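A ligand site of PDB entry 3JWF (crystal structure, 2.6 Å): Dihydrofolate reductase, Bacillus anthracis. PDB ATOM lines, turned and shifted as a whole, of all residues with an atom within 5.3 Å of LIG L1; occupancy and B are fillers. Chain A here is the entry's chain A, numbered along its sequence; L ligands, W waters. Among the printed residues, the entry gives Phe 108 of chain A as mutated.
The backbone carbonyl oxygen (O) of Gly 103 sits at hydrogen-bond distance from the side-chain amide nitrogen (ND2) of Asn 53. The backbone NH of Val 13 lies within hydrogen-bond range of the backbone carbonyl oxygen of Tyr 119 (3.0 Å). The backbone carbonyl oxygen of Phe 102 sits at hydrogen-bond distance from the side-chain amide nitrogen of Asn 53 (3.3 Å). The backbone NH of Thr 121 sits at hydrogen-bond distance from the backbone carbonyl oxygen of Val 13 (2.8 Å). The side-chain hydroxyl (OG1) of Thr 121 lies within hydrogen-bond range of the side-chain carboxylate (OE2) of Glu 34, 2.5 Å away.
Water W1 lies within hydrogen-bond range of the side-chain hydroxyl of Thr 121 (2.7 Å), the backbone carbonyl oxygen of Tyr 119 (3.3 Å), a nitrogen (N3) of LIG L1 (3.3 Å) and the side-chain sulfur of Met 12 (3.7 Å).
Residues that only touch LIG L1: Ile 57 (3.4 Å), Asn 26 (3.4 Å), Val 38 (3.4 Å), Ala 14 (3.5 Å), Thr 121 (3.6 Å), Leu 27 (3.6 Å), Ala 56 (3.7 Å) and Leu 61 (3.8 Å). Hydrophobic or aromatic side chains within 4 Å of LIG L1: Met 12, Ala 14, Leu 27, Val 38, Ala 56, Ile 57, Leu 61 and Phe 102. 13 residues have an atom within 4 Å of LIG L1: Met 12, Val 13, Ala 14, Asn 26, Leu 27, Glu 34, Val 38, Asn 53, Ala 56, Ile 57, Leu 61, Phe 102 and Thr 121. The nearest printed residue that does not touch LIG L1 is Leu 35 (4.02 Å).
An oxygen (O14) of LG2 L2 lies close to a nitrogen (N4) of LIG L1 (3.4 Å).
O12 of LG2 L2 lies within hydrogen-bond range of N of Asn 26. The backbone carbonyl oxygen (O) of Ala 14 is in hydrogen-bond range of a nitrogen (N7) of LG2 L2 (2.8 Å). O of Val 13 is in hydrogen-bond range of N3 of LIG L1 (3.3 Å). The side-chain sulfur of Met 12 sits at hydrogen-bond distance from a nitrogen (N3) of LIG L1 (3.5 Å). OE2 of Glu 34 is in hydrogen-bond range of N3 of LIG L1 (2.8 Å). A nitrogen (N4) of LIG L1 is in hydrogen-bond range of the backbone carbonyl oxygen (O) of Met 12 (2.8 Å). O of Phe 102 sits at hydrogen-bond distance from N4 of LIG L1 (3.3 Å). The side-chain amide oxygen of Asn 53 is in hydrogen-bond range of an oxygen (O1) of LIG L1. The backbone NH (N) of Ala 14 is in hydrogen-bond range of an oxygen (O14) of LG2 L2 (2.8 Å). An oxygen (O2) of LG2 L2 sits close to the backbone NH (N) of Asn 53, 3.1 Å away. The backbone carbonyl oxygen (O) of Asn 26 sits close to an oxygen (O13) of LG2 L2. N2 of LIG L1 sits close to N of Val 13 (3.3 Å).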
ATOM      1  N   MET A  12      10.407 -12.558 -15.174  1.00  0.00           N
ATOM      2  CA  MET A  12       9.401 -11.713 -14.555  1.00  0.00           C
ATOM      3  C   MET A  12       9.236 -12.137 -13.109  1.00  0.00           C
ATOM      4  O   MET A  12       8.756 -13.246 -12.808  1.00  0.00           O
ATOM      5  CB  MET A  12       8.075 -11.805 -15.315  1.00  0.00           C
ATOM      6  CG  MET A  12       6.896 -11.083 -14.662  1.00  0.00           C
ATOM      7  SD  MET A  12       7.092  -9.291 -14.497  1.00  0.00           S
ATOM      8  CE  MET A  12       7.065  -8.764 -16.213  1.00  0.00           C
ATOM      9  N   VAL A  13       9.650 -11.259 -12.195  1.00  0.00           N
ATOM     10  CA  VAL A  13       9.706 -11.607 -10.780  1.00  0.00           C
ATOM     11  C   VAL A  13       9.502 -10.392  -9.887  1.00  0.00           C
ATOM     12  O   VAL A  13       9.888  -9.274 -10.234  1.00  0.00           O
ATOM     13  CB  VAL A  13      11.023 -12.366 -10.429  1.00  0.00           C
ATOM     14  CG1 VAL A  13      12.251 -11.458 -10.555  1.00  0.00           C
ATOM     15  CG2 VAL A  13      10.943 -13.004  -9.047  1.00  0.00           C
ATOM     16  N   ALA A  14       8.881 -10.630  -8.731  1.00  0.00           N
ATOM     17  CA  ALA A  14       8.787  -9.660  -7.650  1.00  0.00           C
ATOM     18  C   ALA A  14       9.377 -10.282  -6.384  1.00  0.00           C
ATOM     19  O   ALA A  14       9.047 -11.403  -6.030  1.00  0.00           O
ATOM     20  CB  ALA A  14       7.354  -9.233  -7.426  1.00  0.00           C
ATOM     21  N   ASN A  25       3.519 -21.776  -0.467  1.00  0.00           N
ATOM     22  CA  ASN A  25       2.994 -21.959  -1.836  1.00  0.00           C
ATOM     23  C   ASN A  25       2.023 -20.860  -2.290  1.00  0.00           C
ATOM     24  O   ASN A  25       1.015 -21.128  -2.960  1.00  0.00           O
ATOM     25  CB  ASN A  25       2.388 -23.357  -2.023  1.00  0.00           C
ATOM     26  CG  ASN A  25       2.890 -24.044  -3.267  1.00  0.00           C
ATOM     27  OD1 ASN A  25       3.895 -23.627  -3.859  1.00  0.00           O
ATOM     28  ND2 ASN A  25       2.216 -25.115  -3.669  1.00  0.00           N
ATOM     29  N   ASN A  26       2.355 -19.615  -1.940  1.00  0.00           N
ATOM     30  CA  ASN A  26       1.518 -18.451  -2.176  1.00  0.00           C
ATOM     31  C   ASN A  26       2.378 -17.179  -2.140  1.00  0.00           C
ATOM     32  O   ASN A  26       3.541 -17.226  -1.739  1.00  0.00           O
ATOM     33  CB  ASN A  26       0.479 -18.369  -1.060  1.00  0.00           C
ATOM     34  CG  ASN A  26      -0.842 -17.757  -1.492  1.00  0.00           C
ATOM     35  OD1 ASN A  26      -0.988 -17.263  -2.632  1.00  0.00           O
ATOM     36  ND2 ASN A  26      -1.817 -17.780  -0.588  1.00  0.00           N
ATOM     37  N   LEU A  27       1.788 -16.063  -2.549  1.00  0.00           N
ATOM     38  CA  LEU A  27       2.416 -14.746  -2.463  1.00  0.00           C
ATOM     39  C   LEU A  27       2.296 -14.184  -1.052  1.00  0.00           C
ATOM     40  O   LEU A  27       1.202 -14.187  -0.467  1.00  0.00           O
ATOM     41  CB  LEU A  27       1.767 -13.797  -3.466  1.00  0.00           C
ATOM     42  CG  LEU A  27       2.305 -13.639  -4.907  1.00  0.00           C
ATOM     43  CD1 LEU A  27       3.142 -14.824  -5.414  1.00  0.00           C
ATOM     44  CD2 LEU A  27       1.160 -13.326  -5.855  1.00  0.00           C
ATOM     45  N   TRP A  29       2.459 -11.111  -0.198  1.00  0.00           N
ATOM     46  CA  TRP A  29       1.887  -9.771  -0.262  1.00  0.00           C
ATOM     47  C   TRP A  29       0.788  -9.689  -1.318  1.00  0.00           C
ATOM     48  O   TRP A  29       0.823 -10.434  -2.305  1.00  0.00           O
ATOM     49  CB  TRP A  29       2.974  -8.738  -0.603  1.00  0.00           C
ATOM     50  CG  TRP A  29       3.725  -9.100  -1.858  1.00  0.00           C
ATOM     51  CD1 TRP A  29       3.336  -8.860  -3.145  1.00  0.00           C
ATOM     52  CD2 TRP A  29       4.975  -9.789  -1.946  1.00  0.00           C
ATOM     53  NE1 TRP A  29       4.266  -9.352  -4.023  1.00  0.00           N
ATOM     54  CE2 TRP A  29       5.279  -9.929  -3.317  1.00  0.00           C
ATOM     55  CE3 TRP A  29       5.869 -10.297  -0.993  1.00  0.00           C
ATOM     56  CZ2 TRP A  29       6.451 -10.565  -3.759  1.00  0.00           C
ATOM     57  CZ3 TRP A  29       7.035 -10.935  -1.443  1.00  0.00           C
ATOM     58  CH2 TRP A  29       7.311 -11.059  -2.808  1.00  0.00           C
ATOM     59  N   GLU A  34       0.795  -3.955  -8.831  1.00  0.00           N
ATOM     60  CA  GLU A  34       1.955  -4.674  -9.314  1.00  0.00           C
ATOM     61  C   GLU A  34       1.519  -5.805 -10.253  1.00  0.00           C
ATOM     62  O   GLU A  34       2.165  -6.022 -11.288  1.00  0.00           O
ATOM     63  CB  GLU A  34       2.755  -5.228  -8.122  1.00  0.00           C
ATOM     64  CG  GLU A  34       4.257  -5.428  -8.368  1.00  0.00           C
ATOM     65  CD  GLU A  34       4.584  -6.712  -9.121  1.00  0.00           C
ATOM     66  OE1 GLU A  34       3.779  -7.676  -9.029  1.00  0.00           O
ATOM     67  OE2 GLU A  34       5.637  -6.770  -9.799  1.00  0.00           O
ATOM     68  N   LEU A  35       0.437  -6.488  -9.896  1.00  0.00           N
ATOM     69  CA  LEU A  35      -0.158  -7.541 -10.722  1.00  0.00           C
ATOM     70  C   LEU A  35      -0.665  -7.027 -12.063  1.00  0.00           C
ATOM     71  O   LEU A  35      -0.643  -7.763 -13.057  1.00  0.00           O
ATOM     72  CB  LEU A  35      -1.298  -8.234  -9.990  1.00  0.00           C
ATOM     73  CG  LEU A  35      -1.042  -9.574  -9.297  1.00  0.00           C
ATOM     74  CD1 LEU A  35      -0.254  -9.426  -7.996  1.00  0.00           C
ATOM     75  CD2 LEU A  35      -2.384 -10.238  -9.022  1.00  0.00           C
ATOM     76  N   VAL A  38       2.300  -6.526 -14.277  1.00  0.00           N
ATOM     77  CA  VAL A  38       2.691  -7.857 -14.735  1.00  0.00           C
ATOM     78  C   VAL A  38       1.860  -8.282 -15.950  1.00  0.00           C
ATOM     79  O   VAL A  38       2.414  -8.740 -16.951  1.00  0.00           O
ATOM     80  CB  VAL A  38       2.593  -8.915 -13.597  1.00  0.00           C
ATOM     81  CG1 VAL A  38       2.882 -10.302 -14.126  1.00  0.00           C
ATOM     82  CG2 VAL A  38       3.576  -8.580 -12.499  1.00  0.00           C
ATOM     83  N   ASN A  53       4.283 -23.596  -9.137  1.00  0.00           N
ATOM     84  CA  ASN A  53       3.806 -22.241  -9.388  1.00  0.00           C
ATOM     85  C   ASN A  53       2.438 -22.259 -10.069  1.00  0.00           C
ATOM     86  O   ASN A  53       1.544 -21.532  -9.658  1.00  0.00           O
ATOM     87  CB  ASN A  53       4.815 -21.403 -10.169  1.00  0.00           C
ATOM     88  CG  ASN A  53       4.347 -19.970 -10.417  1.00  0.00           C
ATOM     89  OD1 ASN A  53       3.532 -19.433  -9.658  1.00  0.00           O
ATOM     90  ND2 ASN A  53       4.839 -19.351 -11.491  1.00  0.00           N
ATOM     91  N   ALA A  56      -0.603 -23.377  -7.723  1.00  0.00           N
ATOM     92  CA  ALA A  56      -0.914 -22.273  -6.805  1.00  0.00           C
ATOM     93  C   ALA A  56      -1.842 -21.241  -7.466  1.00  0.00           C
ATOM     94  O   ALA A  56      -2.808 -20.796  -6.843  1.00  0.00           O
ATOM     95  CB  ALA A  56       0.368 -21.607  -6.319  1.00  0.00           C
ATOM     96  N   ILE A  57      -1.539 -20.884  -8.717  1.00  0.00           N
ATOM     97  CA  ILE A  57      -2.371 -19.978  -9.514  1.00  0.00           C
ATOM     98  C   ILE A  57      -3.736 -20.643  -9.774  1.00  0.00           C
ATOM     99  O   ILE A  57      -4.785 -20.007  -9.594  1.00  0.00           O
ATOM    100  CB  ILE A  57      -1.686 -19.588 -10.853  1.00  0.00           C
ATOM    101  CG1 ILE A  57      -0.422 -18.769 -10.590  1.00  0.00           C
ATOM    102  CG2 ILE A  57      -2.645 -18.812 -11.766  1.00  0.00           C
ATOM    103  CD1 ILE A  57       0.518 -18.686 -11.776  1.00  0.00           C
ATOM    104  N   LEU A  61      -3.753 -18.428 -17.402  1.00  0.00           N
ATOM    105  CA  LEU A  61      -3.785 -16.978 -17.474  1.00  0.00           C
ATOM    106  C   LEU A  61      -4.084 -16.526 -18.907  1.00  0.00           C
ATOM    107  O   LEU A  61      -3.400 -16.936 -19.848  1.00  0.00           O
ATOM    108  CB  LEU A  61      -2.467 -16.392 -16.962  1.00  0.00           C
ATOM    109  CG  LEU A  61      -2.304 -16.411 -15.432  1.00  0.00           C
ATOM    110  CD1 LEU A  61      -0.859 -16.668 -15.022  1.00  0.00           C
ATOM    111  CD2 LEU A  61      -2.832 -15.136 -14.788  1.00  0.00           C
ATOM    112  N   PHE A 102       8.416 -17.183 -15.431  1.00  0.00           N
ATOM    113  CA  PHE A 102       7.439 -16.641 -14.502  1.00  0.00           C
ATOM    114  C   PHE A 102       7.563 -17.212 -13.077  1.00  0.00           C
ATOM    115  O   PHE A 102       6.833 -16.792 -12.169  1.00  0.00           O
ATOM    116  CB  PHE A 102       6.042 -16.882 -15.074  1.00  0.00           C
ATOM    117  CG  PHE A 102       4.995 -15.927 -14.558  1.00  0.00           C
ATOM    118  CD1 PHE A 102       5.159 -14.550 -14.678  1.00  0.00           C
ATOM    119  CD2 PHE A 102       3.838 -16.419 -13.969  1.00  0.00           C
ATOM    120  CE1 PHE A 102       4.186 -13.670 -14.214  1.00  0.00           C
ATOM    121  CE2 PHE A 102       2.856 -15.553 -13.490  1.00  0.00           C
ATOM    122  CZ  PHE A 102       3.034 -14.168 -13.613  1.00  0.00           C
ATOM    123  N   GLY A 103       8.469 -18.165 -12.871  1.00  0.00           N
ATOM    124  CA  GLY A 103       8.695 -18.742 -11.535  1.00  0.00           C
ATOM    125  C   GLY A 103       8.116 -20.130 -11.332  1.00  0.00           C
ATOM    126  O   GLY A 103       7.508 -20.693 -12.248  1.00  0.00           O
ATOM    127  N   PHE A 108      13.177 -20.588 -12.005  1.00  0.00           N
ATOM    128  CA  PHE A 108      14.130 -19.472 -12.146  1.00  0.00           C
ATOM    129  C   PHE A 108      15.575 -19.986 -12.196  1.00  0.00           C
ATOM    130  O   PHE A 108      16.362 -19.516 -13.030  1.00  0.00           O
ATOM    131  CB  PHE A 108      14.002 -18.410 -11.042  1.00  0.00           C
ATOM    132  CG  PHE A 108      12.807 -17.513 -11.164  1.00  0.00           C
ATOM    133  CD1 PHE A 108      12.062 -17.166 -10.034  1.00  0.00           C
ATOM    134  CD2 PHE A 108      12.401 -17.005 -12.398  1.00  0.00           C
ATOM    135  CE1 PHE A 108      10.947 -16.348 -10.143  1.00  0.00           C
ATOM    136  CE2 PHE A 108      11.281 -16.180 -12.518  1.00  0.00           C
ATOM    137  CZ  PHE A 108      10.564 -15.843 -11.381  1.00  0.00           C
ATOM    138  N   TYR A 119      12.892  -8.351 -15.629  1.00  0.00           N
ATOM    139  CA  TYR A 119      11.890  -7.431 -15.084  1.00  0.00           C
ATOM    140  C   TYR A 119      11.662  -7.810 -13.626  1.00  0.00           C
ATOM    141  O   TYR A 119      10.986  -8.808 -13.318  1.00  0.00           O
ATOM    142  CB  TYR A 119      10.565  -7.489 -15.844  1.00  0.00           C
ATOM    143  CG  TYR A 119      10.641  -7.342 -17.357  1.00  0.00           C
ATOM    144  CD1 TYR A 119      11.175  -8.362 -18.143  1.00  0.00           C
ATOM    145  CD2 TYR A 119      10.135  -6.218 -17.996  1.00  0.00           C
ATOM    146  CE1 TYR A 119      11.240  -8.251 -19.522  1.00  0.00           C
ATOM    147  CE2 TYR A 119      10.193  -6.095 -19.373  1.00  0.00           C
ATOM    148  CZ  TYR A 119      10.738  -7.113 -20.129  1.00  0.00           C
ATOM    149  OH  TYR A 119      10.808  -7.018 -21.492  1.00  0.00           O
ATOM    150  N   THR A 121      10.537  -6.545  -9.766  1.00  0.00           N
ATOM    151  CA  THR A 121       9.971  -5.628  -8.801  1.00  0.00           C
ATOM    152  C   THR A 121      10.608  -5.830  -7.428  1.00  0.00           C
ATOM    153  O   THR A 121      10.664  -6.953  -6.904  1.00  0.00           O
ATOM    154  CB  THR A 121       8.438  -5.766  -8.720  1.00  0.00           C
ATOM    155  OG1 THR A 121       7.878  -5.787 -10.035  1.00  0.00           O
ATOM    156  CG2 THR A 121       7.832  -4.607  -7.935  1.00  0.00           C
HETATM  157  N1  LIG L   1       5.091 -10.170  -9.856  1.00  0.00           N
HETATM  158  C1  LIG L   1       6.105 -10.186 -10.738  1.00  0.00           C
HETATM  159  N2  LIG L   1       6.503 -11.329 -11.316  1.00  0.00           N
HETATM  160  C2  LIG L   1       5.881 -12.489 -11.035  1.00  0.00           C
HETATM  161  C3  LIG L   1       4.839 -12.509 -10.116  1.00  0.00           C
HETATM  162  C4  LIG L   1       4.450 -11.305  -9.526  1.00  0.00           C
HETATM  163  C5  LIG L   1      -0.950 -13.847 -11.720  1.00  0.00           C
HETATM  164  C6  LIG L   1      -0.563 -17.942  -5.965  1.00  0.00           C
HETATM  165  C7  LIG L   1      -2.869 -13.918  -7.443  1.00  0.00           C
HETATM  166  C8  LIG L   1       3.301 -11.225  -8.508  1.00  0.00           C
HETATM  167  N3  LIG L   1       6.712  -9.034 -11.016  1.00  0.00           N
HETATM  168  N4  LIG L   1       6.294 -13.615 -11.619  1.00  0.00           N
HETATM  169  O1  LIG L   1       3.089 -16.960 -10.306  1.00  0.00           O
HETATM  170  C9  LIG L   1       4.174 -13.746  -9.796  1.00  0.00           C
HETATM  171  C10 LIG L   1       3.607 -14.802  -9.520  1.00  0.00           C
HETATM  172  C11 LIG L   1       0.672 -15.047  -9.792  1.00  0.00           C
HETATM  173  C12 LIG L   1       0.833 -16.376  -7.796  1.00  0.00           C
HETATM  174  O2  LIG L   1      -1.463 -14.045 -10.383  1.00  0.00           O
HETATM  175  O3  LIG L   1      -1.129 -16.694  -6.418  1.00  0.00           O
HETATM  176  O4  LIG L   1      -2.616 -15.151  -8.149  1.00  0.00           O
HETATM  177  C13 LIG L   1       1.437 -15.827  -8.928  1.00  0.00           C
HETATM  178  C14 LIG L   1      -0.687 -14.816  -9.546  1.00  0.00           C
HETATM  179  C15 LIG L   1      -0.522 -16.169  -7.530  1.00  0.00           C
HETATM  180  C16 LIG L   1      -1.285 -15.372  -8.403  1.00  0.00           C
HETATM  181  C17 LIG L   1       2.933 -16.069  -9.194  1.00  0.00           C
HETATM  182  P1  LG2 L   2       8.270 -24.035  -8.959  1.00  0.00           P
HETATM  183  O1  LG2 L   2       9.659 -23.693  -9.322  1.00  0.00           O
HETATM  184  O2  LG2 L   2       7.302 -23.042  -9.472  1.00  0.00           O
HETATM  185  O3  LG2 L   2       7.906 -25.507  -9.471  1.00  0.00           O
HETATM  186  C1  LG2 L   2       8.735 -26.588  -9.080  1.00  0.00           C
HETATM  187  C2  LG2 L   2       8.374 -27.783  -9.950  1.00  0.00           C
HETATM  188  O4  LG2 L   2       8.869 -27.605 -11.263  1.00  0.00           O
HETATM  189  C3  LG2 L   2       8.962 -29.086  -9.469  1.00  0.00           C
HETATM  190  O5  LG2 L   2       8.166 -29.678  -8.469  1.00  0.00           O
HETATM  191  C4  LG2 L   2       8.935 -29.890 -10.741  1.00  0.00           C
HETATM  192  O6  LG2 L   2       7.613 -30.315 -10.976  1.00  0.00           O
HETATM  193  C5  LG2 L   2       9.251 -28.851 -11.802  1.00  0.00           C
HETATM  194  N1  LG2 L   2      10.692 -28.873 -12.130  1.00  0.00           N
HETATM  195  C6  LG2 L   2      11.733 -28.420 -11.363  1.00  0.00           C
HETATM  196  N2  LG2 L   2      12.883 -28.654 -12.019  1.00  0.00           N
HETATM  197  C7  LG2 L   2      12.604 -29.249 -13.202  1.00  0.00           C
HETATM  198  C8  LG2 L   2      13.398 -29.693 -14.242  1.00  0.00           C
HETATM  199  N3  LG2 L   2      14.716 -29.550 -14.189  1.00  0.00           N
HETATM  200  N4  LG2 L   2      12.820 -30.282 -15.354  1.00  0.00           N
HETATM  201  C9  LG2 L   2      11.446 -30.423 -15.414  1.00  0.00           C
HETATM  202  N5  LG2 L   2      10.666 -29.980 -14.373  1.00  0.00           N
HETATM  203  C10 LG2 L   2      11.225 -29.398 -13.282  1.00  0.00           C
HETATM  204  O7  LG2 L   2       8.141 -24.229  -7.367  1.00  0.00           O
HETATM  205  P2  LG2 L   2       8.830 -23.437  -6.151  1.00  0.00           P
HETATM  206  O8  LG2 L   2       8.435 -24.088  -4.887  1.00  0.00           O
HETATM  207  O9  LG2 L   2      10.258 -23.277  -6.494  1.00  0.00           O
HETATM  208  O10 LG2 L   2       8.146 -21.969  -6.247  1.00  0.00           O
HETATM  209  C11 LG2 L   2       6.784 -21.735  -5.972  1.00  0.00           C
HETATM  210  C12 LG2 L   2       6.676 -20.604  -4.953  1.00  0.00           C
HETATM  211  O11 LG2 L   2       7.196 -19.372  -5.434  1.00  0.00           O
HETATM  212  C13 LG2 L   2       5.228 -20.337  -4.599  1.00  0.00           C
HETATM  213  O12 LG2 L   2       5.236 -19.935  -3.243  1.00  0.00           O
HETATM  214  C14 LG2 L   2       4.859 -19.175  -5.487  1.00  0.00           C
HETATM  215  O13 LG2 L   2       3.819 -18.425  -4.912  1.00  0.00           O
HETATM  216  C15 LG2 L   2       6.159 -18.397  -5.545  1.00  0.00           C
HETATM  217  N6  LG2 L   2       6.335 -17.571  -6.763  1.00  0.00           N
HETATM  218  C16 LG2 L   2       6.626 -16.247  -6.587  1.00  0.00           C
HETATM  219  C17 LG2 L   2       6.837 -15.408  -7.674  1.00  0.00           C
HETATM  220  C18 LG2 L   2       7.224 -13.974  -7.432  1.00  0.00           C
HETATM  221  O14 LG2 L   2       7.668 -13.193  -8.524  1.00  0.00           O
HETATM  222  N7  LG2 L   2       7.137 -13.479  -6.206  1.00  0.00           N
HETATM  223  C19 LG2 L   2       6.745 -15.929  -8.968  1.00  0.00           C
HETATM  224  C20 LG2 L   2       6.453 -17.286  -9.144  1.00  0.00           C
HETATM  225  C21 LG2 L   2       6.247 -18.101  -8.028  1.00  0.00           C
HETATM  226  P3  LG2 L   2       7.120 -31.818 -10.765  1.00  0.00           P
HETATM  227  O15 LG2 L   2       7.982 -32.751 -11.584  1.00  0.00           O
HETATM  228  O16 LG2 L   2       7.242 -32.160  -9.299  1.00  0.00           O
HETATM  229  O17 LG2 L   2       5.685 -31.901 -11.195  1.00  0.00           O
HETATM  230  O   HOH W   1       8.605  -6.682 -12.430  1.00  0.00           O
